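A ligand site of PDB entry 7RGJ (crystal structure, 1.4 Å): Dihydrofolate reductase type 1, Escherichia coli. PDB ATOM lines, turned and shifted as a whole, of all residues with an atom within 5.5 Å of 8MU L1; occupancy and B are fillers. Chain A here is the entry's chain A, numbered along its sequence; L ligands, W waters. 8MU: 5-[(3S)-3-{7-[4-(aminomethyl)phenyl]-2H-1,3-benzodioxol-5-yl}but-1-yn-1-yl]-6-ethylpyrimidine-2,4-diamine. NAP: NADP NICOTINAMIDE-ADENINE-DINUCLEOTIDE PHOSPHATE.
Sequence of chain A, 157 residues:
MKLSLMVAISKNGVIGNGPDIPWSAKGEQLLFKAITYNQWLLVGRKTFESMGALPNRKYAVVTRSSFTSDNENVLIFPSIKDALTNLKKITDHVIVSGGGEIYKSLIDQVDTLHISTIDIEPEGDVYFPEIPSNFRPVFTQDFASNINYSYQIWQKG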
ATOM      1  N   MET A   6     -18.600 -15.545  -8.274  1.00  0.00           N
ATOM      2  CA  MET A   6     -18.884 -15.357  -9.692  1.00  0.00           C
ATOM      3  C   MET A   6     -18.046 -14.214 -10.234  1.00  0.00           C
ATOM      4  O   MET A   6     -18.019 -13.130  -9.639  1.00  0.00           O
ATOM      5  CB  MET A   6     -20.376 -15.079  -9.900  1.00  0.00           C
ATOM      6  CG  MET A   6     -20.769 -15.000 -11.363  1.00  0.00           C
ATOM      7  SD  MET A   6     -22.516 -15.450 -11.589  1.00  0.00           S
ATOM      8  CE  MET A   6     -22.507 -15.870 -13.345  1.00  0.00           C
ATOM      9  N   VAL A   7     -17.389 -14.459 -11.366  1.00  0.00           N
ATOM     10  CA  VAL A   7     -16.465 -13.493 -11.959  1.00  0.00           C
ATOM     11  C   VAL A   7     -16.395 -13.745 -13.456  1.00  0.00           C
ATOM     12  O   VAL A   7     -16.607 -14.875 -13.924  1.00  0.00           O
ATOM     13  CB  VAL A   7     -15.069 -13.652 -11.293  1.00  0.00           C
ATOM     14  CG1 VAL A   7     -14.503 -15.046 -11.558  1.00  0.00           C
ATOM     15  CG2 VAL A   7     -14.120 -12.573 -11.770  1.00  0.00           C
ATOM     16  N   ALA A   8     -16.083 -12.689 -14.204  1.00  0.00           N
ATOM     17  CA  ALA A   8     -15.698 -12.745 -15.602  1.00  0.00           C
ATOM     18  C   ALA A   8     -14.227 -12.358 -15.729  1.00  0.00           C
ATOM     19  O   ALA A   8     -13.843 -11.250 -15.346  1.00  0.00           O
ATOM     20  CB  ALA A   8     -16.557 -11.780 -16.417  1.00  0.00           C
ATOM     21  N   ILE A  21     -14.947  -2.497 -15.670  1.00  0.00           N
ATOM     22  CA  ILE A  21     -14.709  -3.766 -16.345  1.00  0.00           C
ATOM     23  C   ILE A  21     -14.358  -3.436 -17.788  1.00  0.00           C
ATOM     24  O   ILE A  21     -15.182  -2.838 -18.496  1.00  0.00           O
ATOM     25  CB  ILE A  21     -15.923  -4.694 -16.250  1.00  0.00           C
ATOM     26  CG1 ILE A  21     -16.113  -5.112 -14.788  1.00  0.00           C
ATOM     27  CG2 ILE A  21     -15.713  -5.921 -17.122  1.00  0.00           C
ATOM     28  CD1 ILE A  21     -17.352  -5.934 -14.502  1.00  0.00           C
ATOM     29  N   PRO A  22     -13.160  -3.742 -18.247  1.00  0.00           N
ATOM     30  CA  PRO A  22     -12.654  -3.164 -19.498  1.00  0.00           C
ATOM     31  C   PRO A  22     -13.074  -3.909 -20.763  1.00  0.00           C
ATOM     32  O   PRO A  22     -12.255  -4.187 -21.644  1.00  0.00           O
ATOM     33  CB  PRO A  22     -11.133  -3.197 -19.296  1.00  0.00           C
ATOM     34  CG  PRO A  22     -10.916  -4.385 -18.370  1.00  0.00           C
ATOM     35  CD  PRO A  22     -12.113  -4.431 -17.463  1.00  0.00           C
ATOM     36  N   TRP A  23     -14.357  -4.222 -20.868  1.00  0.00           N
ATOM     37  CA  TRP A  23     -14.903  -4.869 -22.053  1.00  0.00           C
ATOM     38  C   TRP A  23     -16.421  -4.845 -21.954  1.00  0.00           C
ATOM     39  O   TRP A  23     -16.989  -4.544 -20.895  1.00  0.00           O
ATOM     40  CB  TRP A  23     -14.428  -6.322 -22.232  1.00  0.00           C
ATOM     41  CG  TRP A  23     -14.840  -7.235 -21.104  1.00  0.00           C
ATOM     42  CD1 TRP A  23     -16.062  -7.820 -20.917  1.00  0.00           C
ATOM     43  CD2 TRP A  23     -14.022  -7.684 -20.024  1.00  0.00           C
ATOM     44  NE1 TRP A  23     -16.051  -8.610 -19.783  1.00  0.00           N
ATOM     45  CE2 TRP A  23     -14.800  -8.522 -19.205  1.00  0.00           C
ATOM     46  CE3 TRP A  23     -12.687  -7.440 -19.655  1.00  0.00           C
ATOM     47  CZ2 TRP A  23     -14.298  -9.125 -18.061  1.00  0.00           C
ATOM     48  CZ3 TRP A  23     -12.195  -8.043 -18.520  1.00  0.00           C
ATOM     49  CH2 TRP A  23     -12.998  -8.882 -17.737  1.00  0.00           C
ATOM     50  N   SER A  24     -17.064  -5.216 -23.057  1.00  0.00           N
ATOM     51  CA  SER A  24     -18.502  -5.456 -23.094  1.00  0.00           C
ATOM     52  C   SER A  24     -18.715  -6.713 -23.924  1.00  0.00           C
ATOM     53  O   SER A  24     -18.468  -6.709 -25.128  1.00  0.00           O
ATOM     54  CB  SER A  24     -19.223  -4.275 -23.742  1.00  0.00           C
ATOM     55  OG  SER A  24     -20.549  -4.649 -24.067  1.00  0.00           O
ATOM     56  N   GLU A  28     -23.128 -11.955 -21.713  1.00  0.00           N
ATOM     57  CA  GLU A  28     -22.500 -12.518 -20.526  1.00  0.00           C
ATOM     58  C   GLU A  28     -23.159 -12.046 -19.241  1.00  0.00           C
ATOM     59  O   GLU A  28     -23.286 -12.830 -18.291  1.00  0.00           O
ATOM     60  CB  GLU A  28     -21.001 -12.228 -20.510  1.00  0.00           C
ATOM     61  CG  GLU A  28     -20.181 -13.208 -19.633  1.00  0.00           C
ATOM     62  CD  GLU A  28     -20.240 -12.909 -18.124  1.00  0.00           C
ATOM     63  OE1 GLU A  28     -20.174 -11.735 -17.725  1.00  0.00           O
ATOM     64  OE2 GLU A  28     -20.394 -13.871 -17.354  1.00  0.00           O
ATOM     65  N   GLN A  29     -23.582 -10.770 -19.202  1.00  0.00           N
ATOM     66  CA  GLN A  29     -24.241 -10.241 -18.009  1.00  0.00           C
ATOM     67  C   GLN A  29     -25.506 -11.011 -17.660  1.00  0.00           C
ATOM     68  O   GLN A  29     -25.909 -11.006 -16.495  1.00  0.00           O
ATOM     69  CB  GLN A  29     -24.550  -8.740 -18.123  1.00  0.00           C
ATOM     70  CG  GLN A  29     -25.084  -8.255 -19.459  1.00  0.00           C
ATOM     71  CD  GLN A  29     -26.552  -8.546 -19.696  1.00  0.00           C
ATOM     72  OE1 GLN A  29     -27.376  -8.511 -18.773  1.00  0.00           O
ATOM     73  NE2 GLN A  29     -26.910  -8.798 -20.956  1.00  0.00           N
ATOM     74  N   LEU A  31     -25.786 -14.190 -17.456  1.00  0.00           N
ATOM     75  CA  LEU A  31     -25.386 -15.244 -16.523  1.00  0.00           C
ATOM     76  C   LEU A  31     -25.316 -14.699 -15.108  1.00  0.00           C
ATOM     77  O   LEU A  31     -25.826 -15.315 -14.159  1.00  0.00           O
ATOM     78  CB  LEU A  31     -24.019 -15.814 -16.921  1.00  0.00           C
ATOM     79  CG  LEU A  31     -24.016 -16.584 -18.251  1.00  0.00           C
ATOM     80  CD1 LEU A  31     -22.599 -16.716 -18.812  1.00  0.00           C
ATOM     81  CD2 LEU A  31     -24.662 -17.969 -18.082  1.00  0.00           C
ATOM     82  N   PHE A  32     -24.683 -13.539 -14.963  1.00  0.00           N
ATOM     83  CA  PHE A  32     -24.586 -12.916 -13.645  1.00  0.00           C
ATOM     84  C   PHE A  32     -25.974 -12.566 -13.103  1.00  0.00           C
ATOM     85  O   PHE A  32     -26.270 -12.821 -11.935  1.00  0.00           O
ATOM     86  CB  PHE A  32     -23.718 -11.659 -13.761  1.00  0.00           C
ATOM     87  CG  PHE A  32     -23.557 -10.910 -12.464  1.00  0.00           C
ATOM     88  CD1 PHE A  32     -22.781 -11.411 -11.447  1.00  0.00           C
ATOM     89  CD2 PHE A  32     -24.222  -9.707 -12.271  1.00  0.00           C
ATOM     90  CE1 PHE A  32     -22.640 -10.724 -10.247  1.00  0.00           C
ATOM     91  CE2 PHE A  32     -24.087  -9.015 -11.065  1.00  0.00           C
ATOM     92  CZ  PHE A  32     -23.297  -9.542 -10.064  1.00  0.00           C
ATOM     93  N   THR A  47     -16.315  -2.017  -5.631  1.00  0.00           N
ATOM     94  CA  THR A  47     -17.236  -2.602  -6.599  1.00  0.00           C
ATOM     95  C   THR A  47     -18.668  -2.148  -6.348  1.00  0.00           C
ATOM     96  O   THR A  47     -19.392  -1.833  -7.309  1.00  0.00           O
ATOM     97  CB  THR A  47     -17.130  -4.124  -6.548  1.00  0.00           C
ATOM     98  OG1 THR A  47     -15.834  -4.523  -7.025  1.00  0.00           O
ATOM     99  CG2 THR A  47     -18.202  -4.779  -7.430  1.00  0.00           C
ATOM    100  N   MET A  51     -20.683  -0.080  -9.070  1.00  0.00           N
ATOM    101  CA  MET A  51     -21.806  -0.742  -9.729  1.00  0.00           C
ATOM    102  C   MET A  51     -23.171  -0.263  -9.245  1.00  0.00           C
ATOM    103  O   MET A  51     -24.142  -0.366  -9.994  1.00  0.00           O
ATOM    104  CB  MET A  51     -21.753  -2.264  -9.536  1.00  0.00           C
ATOM    105  CG  MET A  51     -22.556  -2.729  -8.320  1.00  0.00           C
ATOM    106  SD  MET A  51     -22.268  -4.371  -7.626  1.00  0.00           S
ATOM    107  CE  MET A  51     -23.579  -5.290  -8.442  1.00  0.00           C
ATOM    108  N   LEU A  54     -28.143  -3.296  -8.077  1.00  0.00           N
ATOM    109  CA  LEU A  54     -29.107  -3.879  -9.011  1.00  0.00           C
ATOM    110  C   LEU A  54     -30.394  -4.220  -8.254  1.00  0.00           C
ATOM    111  O   LEU A  54     -30.360  -4.596  -7.088  1.00  0.00           O
ATOM    112  CB  LEU A  54     -28.542  -5.171  -9.604  1.00  0.00           C
ATOM    113  CG  LEU A  54     -27.515  -5.145 -10.735  1.00  0.00           C
ATOM    114  CD1 LEU A  54     -27.148  -6.576 -11.111  1.00  0.00           C
ATOM    115  CD2 LEU A  54     -28.036  -4.392 -11.944  1.00  0.00           C
ATOM    116  N   SER A  97     -19.002 -11.506  -5.151  1.00  0.00           N
ATOM    117  CA  SER A  97     -19.213 -10.871  -6.453  1.00  0.00           C
ATOM    118  C   SER A  97     -18.233  -9.741  -6.730  1.00  0.00           C
ATOM    119  O   SER A  97     -18.508  -8.869  -7.560  1.00  0.00           O
ATOM    120  CB  SER A  97     -20.661 -10.410  -6.602  1.00  0.00           C
ATOM    121  OG  SER A  97     -21.539 -11.483  -6.329  1.00  0.00           O
ATOM    122  N   TYR A 103     -12.156 -11.025  -3.911  1.00  0.00           N
ATOM    123  CA  TYR A 103     -11.875 -12.351  -4.469  1.00  0.00           C
ATOM    124  C   TYR A 103     -10.616 -12.955  -3.859  1.00  0.00           C
ATOM    125  O   TYR A 103     -10.580 -14.160  -3.565  1.00  0.00           O
ATOM    126  CB  TYR A 103     -11.694 -12.272  -5.983  1.00  0.00           C
ATOM    127  CG  TYR A 103     -12.930 -11.970  -6.815  1.00  0.00           C
ATOM    128  CD1 TYR A 103     -14.139 -12.646  -6.605  1.00  0.00           C
ATOM    129  CD2 TYR A 103     -12.856 -11.063  -7.857  1.00  0.00           C
ATOM    130  CE1 TYR A 103     -15.245 -12.392  -7.425  1.00  0.00           C
ATOM    131  CE2 TYR A 103     -13.950 -10.800  -8.657  1.00  0.00           C
ATOM    132  CZ  TYR A 103     -15.134 -11.464  -8.432  1.00  0.00           C
ATOM    133  OH  TYR A 103     -16.197 -11.174  -9.266  1.00  0.00           O
ATOM    134  N   HIS A 114     -18.189 -19.723 -10.399  1.00  0.00           N
ATOM    135  CA  HIS A 114     -18.788 -19.439 -11.698  1.00  0.00           C
ATOM    136  C   HIS A 114     -17.820 -18.518 -12.415  1.00  0.00           C
ATOM    137  O   HIS A 114     -17.702 -17.346 -12.042  1.00  0.00           O
ATOM    138  CB  HIS A 114     -20.114 -18.722 -11.514  1.00  0.00           C
ATOM    139  CG  HIS A 114     -21.157 -19.540 -10.823  1.00  0.00           C
ATOM    140  ND1 HIS A 114     -22.097 -20.281 -11.509  1.00  0.00           N
ATOM    141  CD2 HIS A 114     -21.397 -19.732  -9.513  1.00  0.00           C
ATOM    142  CE1 HIS A 114     -22.876 -20.898 -10.633  1.00  0.00           C
ATOM    143  NE2 HIS A 114     -22.470 -20.588  -9.411  1.00  0.00           N
ATOM    144  N   SER A 116     -16.631 -16.949 -16.082  1.00  0.00           N
ATOM    145  CA  SER A 116     -16.787 -16.682 -17.509  1.00  0.00           C
ATOM    146  C   SER A 116     -15.461 -16.173 -18.057  1.00  0.00           C
ATOM    147  O   SER A 116     -14.980 -15.122 -17.626  1.00  0.00           O
ATOM    148  CB  SER A 116     -17.877 -15.638 -17.741  1.00  0.00           C
ATOM    149  OG  SER A 116     -19.133 -16.179 -17.347  1.00  0.00           O
HETATM  150  C4  8MU L   1     -20.241 -10.122 -14.488  1.00  0.00           C
HETATM  151  C5  8MU L   1     -20.000  -9.904 -13.135  1.00  0.00           C
HETATM  152  C6  8MU L   1     -19.591 -11.004 -12.371  1.00  0.00           C
HETATM  153  N1  8MU L   1     -19.432 -12.201 -12.924  1.00  0.00           N
HETATM  154  N3  8MU L   1     -20.070 -11.346 -15.014  1.00  0.00           N
HETATM  155  C2  8MU L   1     -19.687 -12.368 -14.248  1.00  0.00           C
HETATM  156  CAG 8MU L   1     -20.178  -8.640 -12.536  1.00  0.00           C
HETATM  157  CAH 8MU L   1     -20.316  -7.618 -12.048  1.00  0.00           C
HETATM  158  CAI 8MU L   1     -20.514  -6.297 -11.414  1.00  0.00           C
HETATM  159  CAJ 8MU L   1     -19.214  -5.613 -11.021  1.00  0.00           C
HETATM  160  CAK 8MU L   1     -21.223  -5.464 -12.265  1.00  0.00           C
HETATM  161  CAL 8MU L   1     -20.696  -5.145 -13.503  1.00  0.00           C
HETATM  162  CAM 8MU L   1     -21.409  -4.297 -14.338  1.00  0.00           C
HETATM  163  CAN 8MU L   1     -20.839  -3.979 -15.580  1.00  0.00           C
HETATM  164  CAO 8MU L   1     -20.414  -4.971 -16.463  1.00  0.00           C
HETATM  165  CAP 8MU L   1     -19.852  -4.632 -17.697  1.00  0.00           C
HETATM  166  CAQ 8MU L   1     -19.675  -3.295 -18.059  1.00  0.00           C
HETATM  167  CAR 8MU L   1     -19.099  -2.945 -19.317  1.00  0.00           C
HETATM  168  CAT 8MU L   1     -20.083  -2.308 -17.173  1.00  0.00           C
HETATM  169  CAU 8MU L   1     -20.662  -2.642 -15.943  1.00  0.00           C
HETATM  170  CAV 8MU L   1     -22.585  -3.797 -13.933  1.00  0.00           C
HETATM  171  CAX 8MU L   1     -24.365  -2.522 -13.596  1.00  0.00           C
HETATM  172  CAZ 8MU L   1     -23.103  -4.108 -12.737  1.00  0.00           C
HETATM  173  CBA 8MU L   1     -22.454  -4.927 -11.903  1.00  0.00           C
HETATM  174  CBC 8MU L   1     -20.664  -9.097 -15.336  1.00  0.00           C
HETATM  175  CBD 8MU L   1     -19.492  -8.649 -16.201  1.00  0.00           C
HETATM  176  NAA 8MU L   1     -19.540 -13.566 -14.767  1.00  0.00           N
HETATM  177  NAE 8MU L   1     -19.331 -10.816 -11.070  1.00  0.00           N
HETATM  178  NAS 8MU L   1     -17.874  -2.119 -19.252  1.00  0.00           N
HETATM  179  OAW 8MU L   1     -23.433  -2.961 -14.601  1.00  0.00           O
HETATM  180  OAY 8MU L   1     -24.312  -3.506 -12.541  1.00  0.00           O
HETATM  181  PA  NAP L   2     -13.056  -4.173  -4.221  1.00  0.00           P
HETATM  182  O1A NAP L   2     -12.596  -5.532  -3.885  1.00  0.00           O
HETATM  183  O2A NAP L   2     -14.367  -4.109  -4.975  1.00  0.00           O
HETATM  184  O5B NAP L   2     -13.259  -3.257  -2.862  1.00  0.00           O
HETATM  185  C5B NAP L   2     -12.084  -2.883  -2.172  1.00  0.00           C
HETATM  186  C4B NAP L   2     -12.524  -2.090  -0.918  1.00  0.00           C
HETATM  187  O4B NAP L   2     -13.400  -3.111  -0.045  1.00  0.00           O
HETATM  188  C3B NAP L   2     -11.571  -1.799  -0.139  1.00  0.00           C
HETATM  189  O3B NAP L   2     -10.971  -0.525  -0.516  1.00  0.00           O
HETATM  190  C2B NAP L   2     -12.349  -1.648   1.340  1.00  0.00           C
HETATM  191  O2B NAP L   2     -13.250  -0.549   1.314  1.00  0.00           O
HETATM  192  C1B NAP L   2     -13.085  -2.731   1.407  1.00  0.00           C
HETATM  193  N9A NAP L   2     -12.379  -3.886   1.968  1.00  0.00           N
HETATM  194  C8A NAP L   2     -11.579  -4.761   1.374  1.00  0.00           C
HETATM  195  N7A NAP L   2     -11.162  -5.671   2.235  1.00  0.00           N
HETATM  196  C5A NAP L   2     -11.727  -5.368   3.427  1.00  0.00           C
HETATM  197  C6A NAP L   2     -11.703  -5.919   4.719  1.00  0.00           C
HETATM  198  N6A NAP L   2     -10.923  -7.094   5.021  1.00  0.00           N
HETATM  199  N1A NAP L   2     -12.437  -5.323   5.643  1.00  0.00           N
HETATM  200  C2A NAP L   2     -13.172  -4.240   5.423  1.00  0.00           C
HETATM  201  N3A NAP L   2     -13.230  -3.672   4.222  1.00  0.00           N
HETATM  202  C4A NAP L   2     -12.509  -4.243   3.241  1.00  0.00           C
HETATM  203  O3  NAP L   2     -11.907  -3.294  -5.002  1.00  0.00           O
HETATM  204  PN  NAP L   2     -10.854  -3.790  -6.132  1.00  0.00           P
HETATM  205  O1N NAP L   2     -10.087  -2.577  -6.602  1.00  0.00           O
HETATM  206  O2N NAP L   2      -9.990  -4.923  -5.679  1.00  0.00           O
HETATM  207  O5D NAP L   2     -11.848  -4.340  -7.345  1.00  0.00           O
HETATM  208  C5D NAP L   2     -12.571  -3.427  -8.155  1.00  0.00           C
HETATM  209  C4D NAP L   2     -12.344  -3.809  -9.495  1.00  0.00           C
HETATM  210  O4D NAP L   2     -12.848  -5.219  -9.756  1.00  0.00           O
HETATM  211  C3D NAP L   2     -13.104  -2.915 -10.560  1.00  0.00           C
HETATM  212  O3D NAP L   2     -12.120  -2.704 -11.696  1.00  0.00           O
HETATM  213  C2D NAP L   2     -14.094  -3.608 -10.894  1.00  0.00           C
HETATM  214  O2D NAP L   2     -14.539  -3.324 -12.278  1.00  0.00           O
HETATM  215  C1D NAP L   2     -13.528  -5.161 -10.844  1.00  0.00           C
HETATM  216  N1N NAP L   2     -14.573  -6.141 -10.832  1.00  0.00           N
HETATM  217  C2N NAP L   2     -14.591  -7.086 -11.899  1.00  0.00           C
HETATM  218  C3N NAP L   2     -15.641  -8.171 -11.931  1.00  0.00           C
HETATM  219  C7N NAP L   2     -15.595  -9.174 -13.039  1.00  0.00           C
HETATM  220  O7N NAP L   2     -16.274 -10.135 -12.965  1.00  0.00           O
HETATM  221  N7N NAP L   2     -14.712  -8.900 -14.155  1.00  0.00           N
HETATM  222  C4N NAP L   2     -16.704  -8.310 -10.850  1.00  0.00           C
HETATM  223  C5N NAP L   2     -16.601  -7.247  -9.764  1.00  0.00           C
HETATM  224  C6N NAP L   2     -15.552  -6.181  -9.796  1.00  0.00           C
HETATM  225  P2B NAP L   2     -12.843   0.954   1.843  1.00  0.00           P
HETATM  226  O1X NAP L   2     -11.802   1.488   0.884  1.00  0.00           O
HETATM  227  O2X NAP L   2     -12.276   0.854   3.252  1.00  0.00           O
HETATM  228  O3X NAP L   2     -14.084   1.789   1.825  1.00  0.00           O
HETATM  229  O   HOH W   1     -18.522 -10.000 -19.139  1.00  0.00           O
HETATM  230  O   HOH W   2     -16.989  -0.458 -17.358  1.00  0.00           O
HETATM  231  O   HOH W   3     -19.385 -16.430 -14.401  1.00  0.00           O
HETATM  232  O   HOH W   4     -17.692  -1.363 -15.188  1.00  0.00           O
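The backbone carbonyl oxygen (O) of Met 6 is in hydrogen-bond range of the side-chain hydroxyl (OH) of Tyr 103. The side-chain hydroxyl (OG) of Ser 116 sits at hydrogen-bond distance from the side-chain carboxylate (OE2) of Glu 28, at 2.6 Å. O of Val 7 is in hydrogen-bond range of N of Ser 116 (3.0 Å). N of Val 7 is in hydrogen-bond range of O of His 114.
Merely in contact with 8MU L1: Phe 32, Ala 8, Met 51, Tyr 103, Ser 116, Thr 47 and Leu 54. Hydrophobic or aromatic side chains within 4 Å of 8MU L1: Met 6, Ala 8, Ile 21, Phe 32, Met 51 and Leu 54. 12 residues have an atom within 4 Å of 8MU L1: Met 6, Val 7, Ala 8, Ile 21, Trp 23, Glu 28, Phe 32, Thr 47, Met 51, Leu 54, Tyr 103 and Ser 116.
The backbone carbonyl oxygen (O) of Met 6 is in hydrogen-bond range of a nitrogen (NAE) of 8MU L1 (3.0 Å). N of Thr 47 lies within hydrogen-bond range of O2A of NAP L2, 2.9 Å away. An oxygen (O7N) of NAP L2 sits at hydrogen-bond distance from the backbone NH (N) of Ala 8 (2.8 Å). O of Ala 8 lies within hydrogen-bond range of N7N of NAP L2 (2.8 Å). A nitrogen (NAA) of 8MU L1 sits at hydrogen-bond distance from the backbone carbonyl oxygen of Val 7, at 3.3 Å. OG1 of Thr 47 sits at hydrogen-bond distance from O2A of NAP L2, at 2.6 Å. N1 of 8MU L1 lies close to N of Val 7, at 3.4 Å. The backbone carbonyl oxygen of Trp 23 sits at hydrogen-bond distance from a nitrogen (NAS) of 8MU L1. O of Ile 21 lies within hydrogen-bond range of NAS of 8MU L1. A nitrogen (N3) of 8MU L1 is in hydrogen-bond range of the side-chain carboxylate (OE1) of Glu 28.
Water W2 lies within hydrogen-bond range of a nitrogen (NAS) of 8MU L1 (2.7 Å) and the backbone carbonyl oxygen (O) of Ile 21 (3.2 Å). Water W3 lies within hydrogen-bond range of a nitrogen (NAA) of 8MU L1 (2.9 Å), the side-chain hydroxyl (OG) of Ser 116 (3.0 Å), the backbone carbonyl oxygen (O) of His 114 (3.0 Å) and the backbone carbonyl oxygen (O) of Val 7 (3.2 Å). Water W1 lies within hydrogen-bond range of OE1 of Glu 28 (2.8 Å) and NE1 of Trp 23 (2.9 Å).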
